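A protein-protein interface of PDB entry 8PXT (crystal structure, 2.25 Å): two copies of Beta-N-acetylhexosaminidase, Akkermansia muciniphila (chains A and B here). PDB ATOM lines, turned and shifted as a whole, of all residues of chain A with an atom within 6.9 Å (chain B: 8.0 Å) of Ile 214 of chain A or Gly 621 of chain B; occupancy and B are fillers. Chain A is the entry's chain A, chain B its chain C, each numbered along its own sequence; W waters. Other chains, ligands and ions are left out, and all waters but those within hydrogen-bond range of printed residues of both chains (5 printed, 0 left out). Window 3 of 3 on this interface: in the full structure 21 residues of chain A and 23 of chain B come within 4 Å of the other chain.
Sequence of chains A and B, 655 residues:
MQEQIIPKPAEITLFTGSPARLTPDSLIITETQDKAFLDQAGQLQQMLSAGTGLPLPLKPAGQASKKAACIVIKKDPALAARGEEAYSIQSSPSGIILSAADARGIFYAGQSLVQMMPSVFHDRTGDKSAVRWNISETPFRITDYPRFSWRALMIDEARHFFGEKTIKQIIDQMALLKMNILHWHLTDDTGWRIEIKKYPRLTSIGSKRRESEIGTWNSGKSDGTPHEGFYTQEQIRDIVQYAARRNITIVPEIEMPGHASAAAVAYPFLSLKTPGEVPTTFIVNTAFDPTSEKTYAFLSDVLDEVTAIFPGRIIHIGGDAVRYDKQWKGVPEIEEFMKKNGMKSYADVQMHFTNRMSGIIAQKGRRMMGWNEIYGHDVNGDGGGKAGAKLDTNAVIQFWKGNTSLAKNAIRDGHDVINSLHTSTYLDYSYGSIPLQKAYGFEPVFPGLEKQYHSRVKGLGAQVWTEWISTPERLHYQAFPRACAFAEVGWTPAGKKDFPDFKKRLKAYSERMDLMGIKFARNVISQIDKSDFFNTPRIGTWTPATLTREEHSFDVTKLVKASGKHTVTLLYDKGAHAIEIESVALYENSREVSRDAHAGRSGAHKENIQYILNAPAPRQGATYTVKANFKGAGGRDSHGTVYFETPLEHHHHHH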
ATOM      1  N   HIS A 160      11.521 -25.711 -39.067  1.00  0.00           N
ATOM      2  CA  HIS A 160      11.857 -27.086 -39.406  1.00  0.00           C
ATOM      3  C   HIS A 160      12.160 -27.146 -40.894  1.00  0.00           C
ATOM      4  O   HIS A 160      11.439 -26.557 -41.704  1.00  0.00           O
ATOM      5  CB  HIS A 160      10.727 -28.066 -39.066  1.00  0.00           C
ATOM      6  CG  HIS A 160      10.643 -28.419 -37.614  1.00  0.00           C
ATOM      7  ND1 HIS A 160       9.842 -27.734 -36.727  1.00  0.00           N
ATOM      8  CD2 HIS A 160      11.259 -29.387 -36.894  1.00  0.00           C
ATOM      9  CE1 HIS A 160       9.965 -28.266 -35.523  1.00  0.00           C
ATOM     10  NE2 HIS A 160      10.820 -29.270 -35.597  1.00  0.00           N
ATOM     11  N   SER A 212      14.644 -29.627 -30.252  1.00  0.00           N
ATOM     12  CA  SER A 212      13.530 -28.740 -30.561  1.00  0.00           C
ATOM     13  C   SER A 212      12.452 -28.837 -29.491  1.00  0.00           C
ATOM     14  O   SER A 212      12.045 -29.937 -29.105  1.00  0.00           O
ATOM     15  CB  SER A 212      12.917 -29.071 -31.929  1.00  0.00           C
ATOM     16  OG  SER A 212      13.890 -29.009 -32.956  1.00  0.00           O
ATOM     17  N   GLU A 213      12.011 -27.676 -29.016  1.00  0.00           N
ATOM     18  CA  GLU A 213      10.775 -27.574 -28.250  1.00  0.00           C
ATOM     19  C   GLU A 213       9.617 -28.140 -29.067  1.00  0.00           C
ATOM     20  O   GLU A 213       9.563 -27.973 -30.287  1.00  0.00           O
ATOM     21  CB  GLU A 213      10.543 -26.099 -27.900  1.00  0.00           C
ATOM     22  CG  GLU A 213       9.341 -25.766 -27.039  1.00  0.00           C
ATOM     23  CD  GLU A 213       9.181 -24.257 -26.843  1.00  0.00           C
ATOM     24  OE1 GLU A 213       9.406 -23.497 -27.811  1.00  0.00           O
ATOM     25  OE2 GLU A 213       8.844 -23.824 -25.722  1.00  0.00           O
ATOM     26  N   ILE A 214       8.695 -28.838 -28.397  1.00  0.00           N
ATOM     27  CA  ILE A 214       7.547 -29.443 -29.064  1.00  0.00           C
ATOM     28  C   ILE A 214       6.270 -29.125 -28.291  1.00  0.00           C
ATOM     29  O   ILE A 214       6.297 -28.616 -27.171  1.00  0.00           O
ATOM     30  CB  ILE A 214       7.694 -30.972 -29.226  1.00  0.00           C
ATOM     31  CG1 ILE A 214       7.799 -31.644 -27.851  1.00  0.00           C
ATOM     32  CG2 ILE A 214       8.890 -31.296 -30.114  1.00  0.00           C
ATOM     33  CD1 ILE A 214       7.862 -33.158 -27.903  1.00  0.00           C
ATOM     34  N   GLY A 215       5.141 -29.455 -28.911  1.00  0.00           N
ATOM     35  CA  GLY A 215       3.847 -29.222 -28.305  1.00  0.00           C
ATOM     36  C   GLY A 215       3.355 -27.810 -28.545  1.00  0.00           C
ATOM     37  O   GLY A 215       2.431 -27.589 -29.335  1.00  0.00           O
ATOM     38  N   THR A 216       3.975 -26.845 -27.875  1.00  0.00           N
ATOM     39  CA  THR A 216       3.603 -25.444 -28.017  1.00  0.00           C
ATOM     40  C   THR A 216       4.645 -24.596 -27.306  1.00  0.00           C
ATOM     41  O   THR A 216       5.541 -25.109 -26.630  1.00  0.00           O
ATOM     42  CB  THR A 216       2.212 -25.163 -27.446  1.00  0.00           C
ATOM     43  OG1 THR A 216       1.839 -23.812 -27.741  1.00  0.00           O
ATOM     44  CG2 THR A 216       2.203 -25.364 -25.936  1.00  0.00           C
ATOM     45  N   TRP A 217       4.506 -23.284 -27.462  1.00  0.00           N
ATOM     46  CA  TRP A 217       5.411 -22.349 -26.810  1.00  0.00           C
ATOM     47  C   TRP A 217       5.353 -22.528 -25.298  1.00  0.00           C
ATOM     48  O   TRP A 217       4.271 -22.632 -24.715  1.00  0.00           O
ATOM     49  CB  TRP A 217       5.040 -20.916 -27.196  1.00  0.00           C
ATOM     50  CG  TRP A 217       5.227 -20.612 -28.661  1.00  0.00           C
ATOM     51  CD1 TRP A 217       6.393 -20.265 -29.282  1.00  0.00           C
ATOM     52  CD2 TRP A 217       4.219 -20.624 -29.681  1.00  0.00           C
ATOM     53  NE1 TRP A 217       6.175 -20.063 -30.622  1.00  0.00           N
ATOM     54  CE2 TRP A 217       4.849 -20.275 -30.893  1.00  0.00           C
ATOM     55  CE3 TRP A 217       2.848 -20.895 -29.688  1.00  0.00           C
ATOM     56  CZ2 TRP A 217       4.152 -20.190 -32.101  1.00  0.00           C
ATOM     57  CZ3 TRP A 217       2.158 -20.811 -30.886  1.00  0.00           C
ATOM     58  CH2 TRP A 217       2.812 -20.460 -32.076  1.00  0.00           C
ATOM     59  N   ASN A 218       6.524 -22.572 -24.664  1.00  0.00           N
ATOM     60  CA  ASN A 218       6.650 -22.741 -23.217  1.00  0.00           C
ATOM     61  C   ASN A 218       6.083 -24.072 -22.735  1.00  0.00           C
ATOM     62  O   ASN A 218       5.696 -24.198 -21.567  1.00  0.00           O
ATOM     63  CB  ASN A 218       5.969 -21.597 -22.457  1.00  0.00           C
ATOM     64  CG  ASN A 218       6.276 -20.241 -23.048  1.00  0.00           C
ATOM     65  OD1 ASN A 218       5.372 -19.515 -23.465  1.00  0.00           O
ATOM     66  ND2 ASN A 218       7.553 -19.887 -23.087  1.00  0.00           N
ATOM     67  N   SER A 219       6.013 -25.074 -23.615  1.00  0.00           N
ATOM     68  CA  SER A 219       5.522 -26.383 -23.200  1.00  0.00           C
ATOM     69  C   SER A 219       6.412 -27.002 -22.135  1.00  0.00           C
ATOM     70  O   SER A 219       5.949 -27.836 -21.349  1.00  0.00           O
ATOM     71  CB  SER A 219       5.448 -27.323 -24.402  1.00  0.00           C
ATOM     72  OG  SER A 219       6.748 -27.564 -24.913  1.00  0.00           O
ATOM     73  N   GLY A 220       7.683 -26.614 -22.091  1.00  0.00           N
ATOM     74  CA  GLY A 220       8.642 -27.345 -21.288  1.00  0.00           C
ATOM     75  C   GLY A 220       8.981 -28.715 -21.828  1.00  0.00           C
ATOM     76  O   GLY A 220       9.661 -29.484 -21.146  1.00  0.00           O
ATOM     77  N   LYS A 221       8.519 -29.042 -23.033  1.00  0.00           N
ATOM     78  CA  LYS A 221       8.752 -30.333 -23.659  1.00  0.00           C
ATOM     79  C   LYS A 221       9.764 -30.193 -24.787  1.00  0.00           C
ATOM     80  O   LYS A 221       9.823 -29.166 -25.472  1.00  0.00           O
ATOM     81  CB  LYS A 221       7.455 -30.923 -24.218  1.00  0.00           C
ATOM     82  CG  LYS A 221       6.398 -31.225 -23.176  1.00  0.00           C
ATOM     83  CD  LYS A 221       5.181 -31.856 -23.831  1.00  0.00           C
ATOM     84  CE  LYS A 221       3.977 -31.843 -22.911  1.00  0.00           C
ATOM     85  NZ  LYS A 221       2.848 -32.611 -23.497  1.00  0.00           N
ATOM     86  N   SER A 222      10.543 -31.252 -24.984  1.00  0.00           N
ATOM     87  CA  SER A 222      11.598 -31.284 -25.984  1.00  0.00           C
ATOM     88  C   SER A 222      11.645 -32.670 -26.603  1.00  0.00           C
ATOM     89  O   SER A 222      11.293 -33.662 -25.960  1.00  0.00           O
ATOM     90  CB  SER A 222      12.958 -30.938 -25.367  1.00  0.00           C
ATOM     91  OG  SER A 222      14.005 -31.124 -26.302  1.00  0.00           O
ATOM     92  N   ASP A 223      12.082 -32.734 -27.861  1.00  0.00           N
ATOM     93  CA  ASP A 223      12.261 -34.015 -28.534  1.00  0.00           C
ATOM     94  C   ASP A 223      13.669 -34.578 -28.368  1.00  0.00           C
ATOM     95  O   ASP A 223      13.906 -35.727 -28.758  1.00  0.00           O
ATOM     96  CB  ASP A 223      11.921 -33.887 -30.028  1.00  0.00           C
ATOM     97  CG  ASP A 223      12.863 -32.958 -30.780  1.00  0.00           C
ATOM     98  OD1 ASP A 223      13.855 -32.478 -30.188  1.00  0.00           O
ATOM     99  OD2 ASP A 223      12.605 -32.710 -31.980  1.00  0.00           O
ATOM    100  N   GLY A 224      14.595 -33.810 -27.796  1.00  0.00           N
ATOM    101  CA  GLY A 224      15.947 -34.283 -27.558  1.00  0.00           C
ATOM    102  C   GLY A 224      16.597 -34.866 -28.795  1.00  0.00           C
ATOM    103  O   GLY A 224      17.397 -35.803 -28.705  1.00  0.00           O
ATOM    104  N   THR A 280      17.199 -23.751 -29.007  1.00  0.00           N
ATOM    105  CA  THR A 280      16.433 -24.987 -29.056  1.00  0.00           C
ATOM    106  C   THR A 280      14.953 -24.771 -28.781  1.00  0.00           C
ATOM    107  O   THR A 280      14.161 -25.703 -28.956  1.00  0.00           O
ATOM    108  CB  THR A 280      16.990 -25.991 -28.044  1.00  0.00           C
ATOM    109  OG1 THR A 280      16.858 -25.460 -26.722  1.00  0.00           O
ATOM    110  CG2 THR A 280      18.459 -26.274 -28.325  1.00  0.00           C
ATOM    111  N   PHE A 282      11.476 -22.049 -29.401  1.00  0.00           N
ATOM    112  CA  PHE A 282      10.941 -21.127 -30.393  1.00  0.00           C
ATOM    113  C   PHE A 282      10.504 -19.805 -29.775  1.00  0.00           C
ATOM    114  O   PHE A 282       9.718 -19.070 -30.381  1.00  0.00           O
ATOM    115  CB  PHE A 282       9.781 -21.786 -31.143  1.00  0.00           C
ATOM    116  CG  PHE A 282      10.182 -23.029 -31.889  1.00  0.00           C
ATOM    117  CD1 PHE A 282      10.945 -22.943 -33.039  1.00  0.00           C
ATOM    118  CD2 PHE A 282       9.808 -24.280 -31.432  1.00  0.00           C
ATOM    119  CE1 PHE A 282      11.318 -24.075 -33.725  1.00  0.00           C
ATOM    120  CE2 PHE A 282      10.182 -25.420 -32.115  1.00  0.00           C
ATOM    121  CZ  PHE A 282      10.937 -25.316 -33.263  1.00  0.00           C
ATOM    122  N   GLU A 467       6.908 -24.096 -36.532  1.00  0.00           N
ATOM    123  CA  GLU A 467       7.342 -24.426 -35.177  1.00  0.00           C
ATOM    124  C   GLU A 467       6.894 -25.832 -34.797  1.00  0.00           C
ATOM    125  O   GLU A 467       7.677 -26.628 -34.266  1.00  0.00           O
ATOM    126  CB  GLU A 467       6.789 -23.423 -34.162  1.00  0.00           C
ATOM    127  CG  GLU A 467       7.515 -22.097 -34.103  1.00  0.00           C
ATOM    128  CD  GLU A 467       6.932 -21.063 -35.050  1.00  0.00           C
ATOM    129  OE1 GLU A 467       6.181 -21.449 -35.972  1.00  0.00           O
ATOM    130  OE2 GLU A 467       7.226 -19.862 -34.865  1.00  0.00           O
ATOM    131  N   TRP A 468       5.630 -26.156 -35.077  1.00  0.00           N
ATOM    132  CA  TRP A 468       4.996 -27.383 -34.610  1.00  0.00           C
ATOM    133  C   TRP A 468       4.726 -28.355 -35.755  1.00  0.00           C
ATOM    134  O   TRP A 468       3.800 -29.167 -35.688  1.00  0.00           O
ATOM    135  CB  TRP A 468       3.715 -27.023 -33.856  1.00  0.00           C
ATOM    136  CG  TRP A 468       3.930 -25.805 -33.016  1.00  0.00           C
ATOM    137  CD1 TRP A 468       3.285 -24.607 -33.117  1.00  0.00           C
ATOM    138  CD2 TRP A 468       4.899 -25.651 -31.969  1.00  0.00           C
ATOM    139  NE1 TRP A 468       3.783 -23.720 -32.189  1.00  0.00           N
ATOM    140  CE2 TRP A 468       4.775 -24.339 -31.472  1.00  0.00           C
ATOM    141  CE3 TRP A 468       5.854 -26.500 -31.402  1.00  0.00           C
ATOM    142  CZ2 TRP A 468       5.572 -23.855 -30.432  1.00  0.00           C
ATOM    143  CZ3 TRP A 468       6.643 -26.019 -30.369  1.00  0.00           C
ATOM    144  CH2 TRP A 468       6.498 -24.709 -29.896  1.00  0.00           C
ATOM    145  N   THR B 557      -1.980 -40.819 -26.131  1.00  0.00           N
ATOM    146  CA  THR B 557      -0.867 -39.994 -26.592  1.00  0.00           C
ATOM    147  C   THR B 557       0.298 -40.849 -27.070  1.00  0.00           C
ATOM    148  O   THR B 557       0.890 -40.581 -28.121  1.00  0.00           O
ATOM    149  CB  THR B 557      -0.400 -39.059 -25.477  1.00  0.00           C
ATOM    150  OG1 THR B 557      -1.466 -38.174 -25.107  1.00  0.00           O
ATOM    151  CG2 THR B 557       0.810 -38.246 -25.937  1.00  0.00           C
ATOM    152  N   ASN B 589      -5.343 -32.394 -28.237  1.00  0.00           N
ATOM    153  CA  ASN B 589      -5.565 -31.426 -27.168  1.00  0.00           C
ATOM    154  C   ASN B 589      -7.073 -31.292 -26.962  1.00  0.00           C
ATOM    155  O   ASN B 589      -7.724 -32.285 -26.618  1.00  0.00           O
ATOM    156  CB  ASN B 589      -4.856 -30.113 -27.500  1.00  0.00           C
ATOM    157  CG  ASN B 589      -3.335 -30.281 -27.544  1.00  0.00           C
ATOM    158  OD1 ASN B 589      -2.758 -30.980 -26.713  1.00  0.00           O
ATOM    159  ND2 ASN B 589      -2.691 -29.667 -28.529  1.00  0.00           N
ATOM    160  N   PRO B 618       0.588 -36.987 -36.366  1.00  0.00           N
ATOM    161  CA  PRO B 618       0.577 -36.497 -34.984  1.00  0.00           C
ATOM    162  C   PRO B 618       1.404 -35.233 -34.814  1.00  0.00           C
ATOM    163  O   PRO B 618       2.464 -35.068 -35.422  1.00  0.00           O
ATOM    164  CB  PRO B 618       1.169 -37.666 -34.188  1.00  0.00           C
ATOM    165  CG  PRO B 618       1.925 -38.464 -35.189  1.00  0.00           C
ATOM    166  CD  PRO B 618       1.135 -38.350 -36.450  1.00  0.00           C
ATOM    167  N   ARG B 619       0.898 -34.333 -33.977  1.00  0.00           N
ATOM    168  CA  ARG B 619       1.661 -33.172 -33.548  1.00  0.00           C
ATOM    169  C   ARG B 619       2.528 -33.567 -32.361  1.00  0.00           C
ATOM    170  O   ARG B 619       2.008 -33.986 -31.322  1.00  0.00           O
ATOM    171  CB  ARG B 619       0.719 -32.035 -33.174  1.00  0.00           C
ATOM    172  CG  ARG B 619       1.406 -30.773 -32.688  1.00  0.00           C
ATOM    173  CD  ARG B 619       0.376 -29.695 -32.537  1.00  0.00           C
ATOM    174  NE  ARG B 619       0.903 -28.452 -31.991  1.00  0.00           N
ATOM    175  CZ  ARG B 619       0.293 -27.281 -32.114  1.00  0.00           C
ATOM    176  NH1 ARG B 619      -0.831 -27.158 -32.801  1.00  0.00           N
ATOM    177  NH2 ARG B 619       0.827 -26.208 -31.540  1.00  0.00           N
ATOM    178  N   GLN B 620       3.844 -33.447 -32.516  1.00  0.00           N
ATOM    179  CA  GLN B 620       4.754 -33.788 -31.433  1.00  0.00           C
ATOM    180  C   GLN B 620       4.362 -33.043 -30.164  1.00  0.00           C
ATOM    181  O   GLN B 620       4.105 -31.836 -30.192  1.00  0.00           O
ATOM    182  CB  GLN B 620       6.196 -33.441 -31.815  1.00  0.00           C
ATOM    183  CG  GLN B 620       6.795 -34.275 -32.935  1.00  0.00           C
ATOM    184  CD  GLN B 620       8.221 -33.858 -33.262  1.00  0.00           C
ATOM    185  OE1 GLN B 620       8.454 -32.801 -33.850  1.00  0.00           O
ATOM    186  NE2 GLN B 620       9.181 -34.684 -32.874  1.00  0.00           N
ATOM    187  N   GLY B 621       4.305 -33.774 -29.051  1.00  0.00           N
ATOM    188  CA  GLY B 621       4.081 -33.177 -27.752  1.00  0.00           C
ATOM    189  C   GLY B 621       2.640 -32.864 -27.417  1.00  0.00           C
ATOM    190  O   GLY B 621       2.365 -32.438 -26.288  1.00  0.00           O
ATOM    191  N   ALA B 622       1.711 -33.041 -28.349  1.00  0.00           N
ATOM    192  CA  ALA B 622       0.307 -32.873 -28.024  1.00  0.00           C
ATOM    193  C   ALA B 622      -0.213 -34.118 -27.317  1.00  0.00           C
ATOM    194  O   ALA B 622       0.403 -35.186 -27.350  1.00  0.00           O
ATOM    195  CB  ALA B 622      -0.517 -32.603 -29.283  1.00  0.00           C
ATOM    196  N   THR B 623      -1.358 -33.973 -26.666  1.00  0.00           N
ATOM    197  CA  THR B 623      -2.034 -35.108 -26.061  1.00  0.00           C
ATOM    198  C   THR B 623      -3.185 -35.533 -26.960  1.00  0.00           C
ATOM    199  O   THR B 623      -3.912 -34.691 -27.494  1.00  0.00           O
ATOM    200  CB  THR B 623      -2.558 -34.780 -24.661  1.00  0.00           C
ATOM    201  OG1 THR B 623      -3.803 -34.087 -24.767  1.00  0.00           O
ATOM    202  CG2 THR B 623      -1.571 -33.915 -23.903  1.00  0.00           C
ATOM    203  N   TYR B 624      -3.337 -36.839 -27.138  1.00  0.00           N
ATOM    204  CA  TYR B 624      -4.429 -37.406 -27.913  1.00  0.00           C
ATOM    205  C   TYR B 624      -5.335 -38.187 -26.979  1.00  0.00           C
ATOM    206  O   TYR B 624      -4.860 -38.985 -26.163  1.00  0.00           O
ATOM    207  CB  TYR B 624      -3.908 -38.289 -29.045  1.00  0.00           C
ATOM    208  CG  TYR B 624      -3.315 -37.462 -30.150  1.00  0.00           C
ATOM    209  CD1 TYR B 624      -4.109 -36.967 -31.171  1.00  0.00           C
ATOM    210  CD2 TYR B 624      -1.969 -37.139 -30.151  1.00  0.00           C
ATOM    211  CE1 TYR B 624      -3.577 -36.192 -32.172  1.00  0.00           C
ATOM    212  CE2 TYR B 624      -1.425 -36.363 -31.150  1.00  0.00           C
ATOM    213  CZ  TYR B 624      -2.233 -35.891 -32.156  1.00  0.00           C
ATOM    214  OH  TYR B 624      -1.695 -35.115 -33.151  1.00  0.00           O
HETATM  215  O   HOH W   1      -0.286 -23.846 -29.413  1.00  0.00           O
HETATM  216  O   HOH W   2       4.692 -31.655 -34.815  1.00  0.00           O
HETATM  217  O   HOH W   3       0.314 -29.412 -28.461  1.00  0.00           O
HETATM  218  O   HOH W   4       5.152 -29.826 -31.926  1.00  0.00           O
HETATM  219  O   HOH W   5      10.672 -31.428 -33.618  1.00  0.00           O
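The backbone NH (N) of Arg 619 of chain B is in hydrogen-bond range of the side-chain hydroxyl (OH) of Tyr 624 of chain B. OG of Ser 219 of chain A is in hydrogen-bond range of O of Ile 214 of chain A, 2.5 Å away. OG of Ser 219 of chain A lies within hydrogen-bond range of N of Lys 221 of chain A (3.0 Å). The backbone NH (N) of Ile 214 of chain A is in hydrogen-bond range of the backbone carbonyl oxygen (O) of Lys 221 of chain A, at 3.2 Å.
No position is printed for both chains. Of the 7 pairs that touch across the chains among the printed residues, none has its exchanged pair printed and touching as well.
Among the printed residues, pairs that only touch across the chains: Trp 468 of chain A with Arg 619 of chain B, Ile 214 of chain A with Gly 621 of chain B, Ile 214 of chain A with Gln 620 of chain B and Gly 215 of chain A with Gly 621 of chain B.
Hydrophobic or aromatic side chains of chain A within 4 Å of the printed part of chain B: Ile 214 and Trp 468. Along chain A the printed residues that touch a printed residue of chain B span positions 214 to 468. Among the printed residues, 7 pairs touch across the chains. Among the printed residues, no Asp or Glu carboxylate lies within 4 Å of a Lys or Arg side-chain nitrogen of the other chain.
Water W5 lies within hydrogen-bond range of the side-chain amide oxygen (OE1) of Gln 620 of chain B, the side-chain carboxylate (OD2) of Asp 223 of chain A and a ring nitrogen (NE2) of His 160 of chain A. Water W1 lies within hydrogen-bond range of the side-chain hydroxyl (OG1) of Thr 216 of chain A (2.7 Å) and the guanidinium group (NH2) of Arg 619 of chain B (3.4 Å). Water W2 bridges the backbone carbonyl oxygen of Trp 468 of chain A and the backbone NH of Gln 620 of chain B. Water W4 lies within hydrogen-bond range of O of Gln 620 of chain B and N of Gly 215 of chain A. Water W3 bridges the backbone carbonyl oxygen of Gly 215 of chain A (2.9 Å) and the side-chain amide nitrogen of Asn 589 of chain B (3.0 Å).
Of chain B, only Gln 620 (3.8 Å) and Gly 621 (3.8 Å) come within 4 Å of Ile 214 of chain A. Of the printed residues of chain B, Gly 215 of chain A touches Arg 619 (3.1 Å), Gln 620 (2.9 Å) and Gly 621 (3.9 Å). Of the printed residues of chain A, Gln 620 of chain B touches Ile 214 (3.8 Å) and Gly 215 (2.9 Å). Of the printed residues of chain B, Trp 468 of chain A touches Arg 619 (3.3 Å). Gly 224 of chain A touches none of the printed residues of chain B.
O of Gly 621 of chain B is in hydrogen-bond range of NZ of Lys 221 of chain A, at 2.8 Å. NH2 of Arg 619 of chain B is in hydrogen-bond range of O of Gly 215 of chain A, 3.1 Å away. O of Gln 620 of chain B lies within hydrogen-bond range of N of Gly 215 of chain A, 2.9 Å away.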
